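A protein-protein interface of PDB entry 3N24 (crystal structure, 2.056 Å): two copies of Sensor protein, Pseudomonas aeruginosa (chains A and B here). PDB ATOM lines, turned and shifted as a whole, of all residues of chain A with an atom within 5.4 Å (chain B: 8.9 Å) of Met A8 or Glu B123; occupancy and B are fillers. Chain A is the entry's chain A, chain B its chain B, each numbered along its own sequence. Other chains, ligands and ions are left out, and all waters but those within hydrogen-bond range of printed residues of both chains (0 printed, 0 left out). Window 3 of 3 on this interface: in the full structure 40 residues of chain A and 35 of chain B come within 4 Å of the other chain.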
ATOM      1  N   GLU A   5      -7.119  -8.934 -32.598  1.00  0.00           N
ATOM      2  CA  GLU A   5      -8.238  -8.150 -32.090  1.00  0.00           C
ATOM      3  C   GLU A   5      -9.485  -9.005 -31.891  1.00  0.00           C
ATOM      4  O   GLU A   5     -10.045  -9.037 -30.798  1.00  0.00           O
ATOM      5  CB  GLU A   5      -8.555  -6.978 -33.023  1.00  0.00           C
ATOM      6  CG  GLU A   5      -9.524  -5.949 -32.436  1.00  0.00           C
ATOM      7  CD  GLU A   5     -10.898  -6.527 -32.115  1.00  0.00           C
ATOM      8  OE1 GLU A   5     -11.532  -7.110 -33.022  1.00  0.00           O
ATOM      9  OE2 GLU A   5     -11.343  -6.396 -30.953  1.00  0.00           O
ATOM     10  N   GLN A   6      -9.925  -9.687 -32.945  1.00  0.00           N
ATOM     11  CA  GLN A   6     -11.177 -10.447 -32.885  1.00  0.00           C
ATOM     12  C   GLN A   6     -11.086 -11.685 -31.990  1.00  0.00           C
ATOM     13  O   GLN A   6     -12.045 -12.043 -31.316  1.00  0.00           O
ATOM     14  CB  GLN A   6     -11.684 -10.791 -34.289  1.00  0.00           C
ATOM     15  CG  GLN A   6     -12.988 -10.075 -34.646  1.00  0.00           C
ATOM     16  CD  GLN A   6     -13.028  -9.586 -36.083  1.00  0.00           C
ATOM     17  OE1 GLN A   6     -11.993  -9.445 -36.736  1.00  0.00           O
ATOM     18  NE2 GLN A   6     -14.230  -9.315 -36.581  1.00  0.00           N
ATOM     19  N   ARG A   7      -9.933 -12.342 -31.999  1.00  0.00           N
ATOM     20  CA  ARG A   7      -9.665 -13.425 -31.063  1.00  0.00           C
ATOM     21  C   ARG A   7      -9.779 -12.870 -29.654  1.00  0.00           C
ATOM     22  O   ARG A   7     -10.338 -13.508 -28.759  1.00  0.00           O
ATOM     23  CB  ARG A   7      -8.253 -13.976 -31.277  1.00  0.00           C
ATOM     24  CG  ARG A   7      -8.189 -15.473 -31.534  1.00  0.00           C
ATOM     25  CD  ARG A   7      -8.840 -16.266 -30.411  1.00  0.00           C
ATOM     26  NE  ARG A   7      -9.109 -17.643 -30.814  1.00  0.00           N
ATOM     27  CZ  ARG A   7      -9.943 -18.460 -30.178  1.00  0.00           C
ATOM     28  NH1 ARG A   7     -10.127 -19.695 -30.622  1.00  0.00           N
ATOM     29  NH2 ARG A   7     -10.598 -18.039 -29.105  1.00  0.00           N
ATOM     30  N   MET A   8      -9.247 -11.665 -29.480  1.00  0.00           N
ATOM     31  CA  MET A   8      -9.211 -10.962 -28.210  1.00  0.00           C
ATOM     32  C   MET A   8     -10.615 -10.557 -27.761  1.00  0.00           C
ATOM     33  O   MET A   8     -10.916 -10.528 -26.570  1.00  0.00           O
ATOM     34  CB  MET A   8      -8.339  -9.725 -28.389  1.00  0.00           C
ATOM     35  CG  MET A   8      -7.894  -9.043 -27.128  1.00  0.00           C
ATOM     36  SD  MET A   8      -6.033  -8.525 -27.333  1.00  0.00           S
ATOM     37  CE  MET A   8      -6.094  -6.827 -26.375  1.00  0.00           C
ATOM     38  N   SER A   9     -11.469 -10.262 -28.734  1.00  0.00           N
ATOM     39  CA  SER A   9     -12.828  -9.788 -28.482  1.00  0.00           C
ATOM     40  C   SER A   9     -13.790 -10.917 -28.096  1.00  0.00           C
ATOM     41  O   SER A   9     -14.789 -10.685 -27.422  1.00  0.00           O
ATOM     42  CB  SER A   9     -13.349  -9.033 -29.713  1.00  0.00           C
ATOM     43  OG  SER A   9     -14.739  -8.784 -29.628  1.00  0.00           O
ATOM     44  N   HIS A  10     -13.499 -12.137 -28.530  1.00  0.00           N
ATOM     45  CA  HIS A  10     -14.309 -13.272 -28.115  1.00  0.00           C
ATOM     46  C   HIS A  10     -13.992 -13.582 -26.651  1.00  0.00           C
ATOM     47  O   HIS A  10     -14.886 -13.844 -25.852  1.00  0.00           O
ATOM     48  CB  HIS A  10     -14.056 -14.500 -28.999  1.00  0.00           C
ATOM     49  CG  HIS A  10     -14.267 -14.251 -30.461  1.00  0.00           C
ATOM     50  ND1 HIS A  10     -13.746 -15.070 -31.438  1.00  0.00           N
ATOM     51  CD2 HIS A  10     -14.932 -13.262 -31.112  1.00  0.00           C
ATOM     52  CE1 HIS A  10     -14.084 -14.603 -32.629  1.00  0.00           C
ATOM     53  NE2 HIS A  10     -14.800 -13.505 -32.460  1.00  0.00           N
ATOM     54  N   HIS A  11     -12.710 -13.531 -26.309  1.00  0.00           N
ATOM     55  CA  HIS A  11     -12.279 -13.753 -24.945  1.00  0.00           C
ATOM     56  C   HIS A  11     -12.900 -12.748 -23.996  1.00  0.00           C
ATOM     57  O   HIS A  11     -13.313 -13.111 -22.905  1.00  0.00           O
ATOM     58  CB  HIS A  11     -10.764 -13.682 -24.849  1.00  0.00           C
ATOM     59  CG  HIS A  11     -10.070 -14.801 -25.551  1.00  0.00           C
ATOM     60  ND1 HIS A  11     -10.296 -16.125 -25.240  1.00  0.00           N
ATOM     61  CD2 HIS A  11      -9.145 -14.798 -26.539  1.00  0.00           C
ATOM     62  CE1 HIS A  11      -9.546 -16.890 -26.011  1.00  0.00           C
ATOM     63  NE2 HIS A  11      -8.837 -16.110 -26.808  1.00  0.00           N
ATOM     64  N   TYR A  12     -12.952 -11.484 -24.411  1.00  0.00           N
ATOM     65  CA  TYR A  12     -13.523 -10.435 -23.575  1.00  0.00           C
ATOM     66  C   TYR A  12     -15.016 -10.615 -23.366  1.00  0.00           C
ATOM     67  O   TYR A  12     -15.525 -10.299 -22.310  1.00  0.00           O
ATOM     68  CB  TYR A  12     -13.263  -9.056 -24.169  1.00  0.00           C
ATOM     69  CG  TYR A  12     -12.052  -8.365 -23.600  1.00  0.00           C
ATOM     70  CD1 TYR A  12     -12.048  -7.898 -22.292  1.00  0.00           C
ATOM     71  CD2 TYR A  12     -10.915  -8.160 -24.379  1.00  0.00           C
ATOM     72  CE1 TYR A  12     -10.940  -7.257 -21.767  1.00  0.00           C
ATOM     73  CE2 TYR A  12      -9.800  -7.518 -23.866  1.00  0.00           C
ATOM     74  CZ  TYR A  12      -9.816  -7.070 -22.559  1.00  0.00           C
ATOM     75  OH  TYR A  12      -8.707  -6.435 -22.043  1.00  0.00           O
ATOM     76  N   ALA A  13     -15.718 -11.109 -24.380  1.00  0.00           N
ATOM     77  CA  ALA A  13     -17.146 -11.394 -24.246  1.00  0.00           C
ATOM     78  C   ALA A  13     -17.381 -12.533 -23.254  1.00  0.00           C
ATOM     79  O   ALA A  13     -18.385 -12.576 -22.566  1.00  0.00           O
ATOM     80  CB  ALA A  13     -17.771 -11.733 -25.631  1.00  0.00           C
ATOM     81  N   ILE A 119      -7.297  -2.679 -19.660  1.00  0.00           N
ATOM     82  CA  ILE A 119      -6.488  -3.390 -20.644  1.00  0.00           C
ATOM     83  C   ILE A 119      -7.143  -3.284 -22.006  1.00  0.00           C
ATOM     84  O   ILE A 119      -6.501  -2.915 -22.994  1.00  0.00           O
ATOM     85  CB  ILE A 119      -6.372  -4.884 -20.300  1.00  0.00           C
ATOM     86  CG1 ILE A 119      -5.491  -5.090 -19.068  1.00  0.00           C
ATOM     87  CG2 ILE A 119      -5.808  -5.657 -21.476  1.00  0.00           C
ATOM     88  CD1 ILE A 119      -5.380  -6.531 -18.655  1.00  0.00           C
ATOM     89  N   TYR B  12      -3.116  -5.540 -15.036  1.00  0.00           N
ATOM     90  CA  TYR B  12      -2.963  -6.965 -14.756  1.00  0.00           C
ATOM     91  C   TYR B  12      -2.690  -7.287 -13.292  1.00  0.00           C
ATOM     92  O   TYR B  12      -3.025  -8.374 -12.812  1.00  0.00           O
ATOM     93  CB  TYR B  12      -1.901  -7.595 -15.657  1.00  0.00           C
ATOM     94  CG  TYR B  12      -2.504  -8.332 -16.819  1.00  0.00           C
ATOM     95  CD1 TYR B  12      -3.295  -9.454 -16.609  1.00  0.00           C
ATOM     96  CD2 TYR B  12      -2.295  -7.907 -18.123  1.00  0.00           C
ATOM     97  CE1 TYR B  12      -3.863 -10.137 -17.668  1.00  0.00           C
ATOM     98  CE2 TYR B  12      -2.857  -8.584 -19.192  1.00  0.00           C
ATOM     99  CZ  TYR B  12      -3.642  -9.697 -18.956  1.00  0.00           C
ATOM    100  OH  TYR B  12      -4.206 -10.377 -20.009  1.00  0.00           O
ATOM    101  N   ALA B 115     -10.497 -17.385 -20.122  1.00  0.00           N
ATOM    102  CA  ALA B 115     -10.617 -16.298 -21.083  1.00  0.00           C
ATOM    103  C   ALA B 115      -9.499 -15.265 -20.915  1.00  0.00           C
ATOM    104  O   ALA B 115      -8.904 -14.822 -21.893  1.00  0.00           O
ATOM    105  CB  ALA B 115     -12.002 -15.635 -20.974  1.00  0.00           C
ATOM    106  N   LEU B 116      -9.213 -14.896 -19.672  1.00  0.00           N
ATOM    107  CA  LEU B 116      -8.171 -13.924 -19.365  1.00  0.00           C
ATOM    108  C   LEU B 116      -6.802 -14.407 -19.835  1.00  0.00           C
ATOM    109  O   LEU B 116      -5.947 -13.607 -20.220  1.00  0.00           O
ATOM    110  CB  LEU B 116      -8.138 -13.670 -17.861  1.00  0.00           C
ATOM    111  CG  LEU B 116      -7.503 -12.362 -17.401  1.00  0.00           C
ATOM    112  CD1 LEU B 116      -8.039 -11.209 -18.226  1.00  0.00           C
ATOM    113  CD2 LEU B 116      -7.746 -12.128 -15.908  1.00  0.00           C
ATOM    114  N   ALA B 117      -6.595 -15.721 -19.791  1.00  0.00           N
ATOM    115  CA  ALA B 117      -5.368 -16.310 -20.306  1.00  0.00           C
ATOM    116  C   ALA B 117      -5.323 -16.134 -21.813  1.00  0.00           C
ATOM    117  O   ALA B 117      -4.337 -15.656 -22.363  1.00  0.00           O
ATOM    118  CB  ALA B 117      -5.289 -17.774 -19.949  1.00  0.00           C
ATOM    119  N   GLY B 118      -6.407 -16.519 -22.474  1.00  0.00           N
ATOM    120  CA  GLY B 118      -6.505 -16.398 -23.916  1.00  0.00           C
ATOM    121  C   GLY B 118      -6.208 -15.003 -24.431  1.00  0.00           C
ATOM    122  O   GLY B 118      -5.873 -14.832 -25.601  1.00  0.00           O
ATOM    123  N   ILE B 119      -6.332 -14.004 -23.561  1.00  0.00           N
ATOM    124  CA  ILE B 119      -6.017 -12.628 -23.929  1.00  0.00           C
ATOM    125  C   ILE B 119      -4.534 -12.303 -23.759  1.00  0.00           C
ATOM    126  O   ILE B 119      -3.904 -11.789 -24.680  1.00  0.00           O
ATOM    127  CB  ILE B 119      -6.854 -11.605 -23.141  1.00  0.00           C
ATOM    128  CG1 ILE B 119      -8.342 -11.792 -23.443  1.00  0.00           C
ATOM    129  CG2 ILE B 119      -6.419 -10.187 -23.490  1.00  0.00           C
ATOM    130  CD1 ILE B 119      -9.222 -10.756 -22.796  1.00  0.00           C
ATOM    131  N   SER B 120      -3.976 -12.595 -22.585  1.00  0.00           N
ATOM    132  CA  SER B 120      -2.548 -12.374 -22.367  1.00  0.00           C
ATOM    133  C   SER B 120      -1.771 -13.209 -23.378  1.00  0.00           C
ATOM    134  O   SER B 120      -0.642 -12.884 -23.745  1.00  0.00           O
ATOM    135  CB  SER B 120      -2.139 -12.735 -20.934  1.00  0.00           C
ATOM    136  OG  SER B 120      -1.705 -14.082 -20.849  1.00  0.00           O
ATOM    137  N   GLU B 121      -2.402 -14.292 -23.821  1.00  0.00           N
ATOM    138  CA  GLU B 121      -1.892 -15.109 -24.910  1.00  0.00           C
ATOM    139  C   GLU B 121      -1.874 -14.296 -26.198  1.00  0.00           C
ATOM    140  O   GLU B 121      -0.899 -14.315 -26.944  1.00  0.00           O
ATOM    141  CB  GLU B 121      -2.790 -16.332 -25.093  1.00  0.00           C
ATOM    142  CG  GLU B 121      -2.096 -17.666 -24.889  1.00  0.00           C
ATOM    143  CD  GLU B 121      -1.454 -18.181 -26.157  1.00  0.00           C
ATOM    144  OE1 GLU B 121      -1.632 -17.536 -27.216  1.00  0.00           O
ATOM    145  OE2 GLU B 121      -0.780 -19.232 -26.096  1.00  0.00           O
ATOM    146  N   ALA B 122      -2.967 -13.579 -26.448  1.00  0.00           N
ATOM    147  CA  ALA B 122      -3.116 -12.763 -27.650  1.00  0.00           C
ATOM    148  C   ALA B 122      -2.208 -11.533 -27.640  1.00  0.00           C
ATOM    149  O   ALA B 122      -1.595 -11.204 -28.656  1.00  0.00           O
ATOM    150  CB  ALA B 122      -4.571 -12.346 -27.829  1.00  0.00           C
ATOM    151  N   GLU B 123      -2.140 -10.853 -26.498  1.00  0.00           N
ATOM    152  CA  GLU B 123      -1.270  -9.691 -26.346  1.00  0.00           C
ATOM    153  C   GLU B 123       0.162 -10.044 -26.728  1.00  0.00           C
ATOM    154  O   GLU B 123       0.810  -9.320 -27.483  1.00  0.00           O
ATOM    155  CB  GLU B 123      -1.320  -9.156 -24.912  1.00  0.00           C
ATOM    156  CG  GLU B 123      -2.491  -8.221 -24.625  1.00  0.00           C
ATOM    157  CD  GLU B 123      -2.282  -6.824 -25.188  1.00  0.00           C
ATOM    158  OE1 GLU B 123      -3.277  -6.187 -25.594  1.00  0.00           O
ATOM    159  OE2 GLU B 123      -1.121  -6.362 -25.226  1.00  0.00           O
ATOM    160  N   THR B 124       0.646 -11.166 -26.202  1.00  0.00           N
ATOM    161  CA  THR B 124       1.980 -11.663 -26.527  1.00  0.00           C
ATOM    162  C   THR B 124       2.113 -11.980 -28.015  1.00  0.00           C
ATOM    163  O   THR B 124       3.096 -11.601 -28.655  1.00  0.00           O
ATOM    164  CB  THR B 124       2.320 -12.926 -25.704  1.00  0.00           C
ATOM    165  OG1 THR B 124       3.029 -12.550 -24.517  1.00  0.00           O
ATOM    166  CG2 THR B 124       3.181 -13.884 -26.515  1.00  0.00           C
ATOM    167  N   SER B 125       1.111 -12.672 -28.554  1.00  0.00           N
ATOM    168  CA  SER B 125       1.117 -13.116 -29.948  1.00  0.00           C
ATOM    169  C   SER B 125       1.462 -11.992 -30.924  1.00  0.00           C
ATOM    170  O   SER B 125       2.129 -12.221 -31.932  1.00  0.00           O
ATOM    171  CB  SER B 125      -0.234 -13.735 -30.318  1.00  0.00           C
ATOM    172  OG  SER B 125      -0.223 -14.242 -31.642  1.00  0.00           O
ATOM    173  N   ALA B 126       1.003 -10.781 -30.621  1.00  0.00           N
ATOM    174  CA  ALA B 126       1.300  -9.621 -31.454  1.00  0.00           C
ATOM    175  C   ALA B 126       2.778  -9.247 -31.367  1.00  0.00           C
ATOM    176  O   ALA B 126       3.260  -8.391 -32.110  1.00  0.00           O
ATOM    177  CB  ALA B 126       0.426  -8.443 -31.053  1.00  0.00           C
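Tyr A12 touches Ile B119, and with the chains exchanged Ile A119 touches Tyr B12.
Positions printed for both chains: 12 and 119.
Printed residues of chain B that touch a printed residue of chain A: Tyr B12, Ala B115, Gly B118, Ile B119 and Glu B123.
Hydrophobic or aromatic side chains of chain B that line the printed part of chain A: Tyr B12, Ala B115 and Ile B119.
Printed residues of chain A that touch a printed residue of chain B: Met A8, His A11, Tyr A12 and Ile A119.
Hydrophobic or aromatic side chains of chain A within 4 Å of the printed part of chain B: Met A8, His A11, Tyr A12 and Ile A119.
NE2 of His A11 lies close to O of Gly B118 (3.4 Å).
Among the printed residues, merely in contact across the chains: Met A8 with Glu B123 (3.0 Å), His A11 with Ala B115 (3.4 Å), His A11 with Ile B119 (3.4 Å), Tyr A12 with Ile B119 (3.5 Å) and Ile A119 with Tyr B12 (3.3 Å).
NH2 of Arg A7 lies close to NE2 of His A11 (3.5 Å).
The side-chain hydroxyl (OH) of Tyr B12 sits close to the backbone NH (N) of Ser B120, at 3.4 Å.
Printed residues of chain A within 4 Å of Ala B115: His A11.
Printed residues of chain A within 4 Å of Gly B118: His A11 (3.4 Å).
Glu B123 touches just one residue of chain A: Met A8.
Thr B124 touches none of the printed residues of chain A.
Ser B125 touches none of the printed residues of chain A.
The nearest residue of chain B that does not touch Met A8 is Ile B119 (4.1 Å).
The nearest residue of chain A that does not touch Glu B123 is Ile A119 (4.9 Å).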
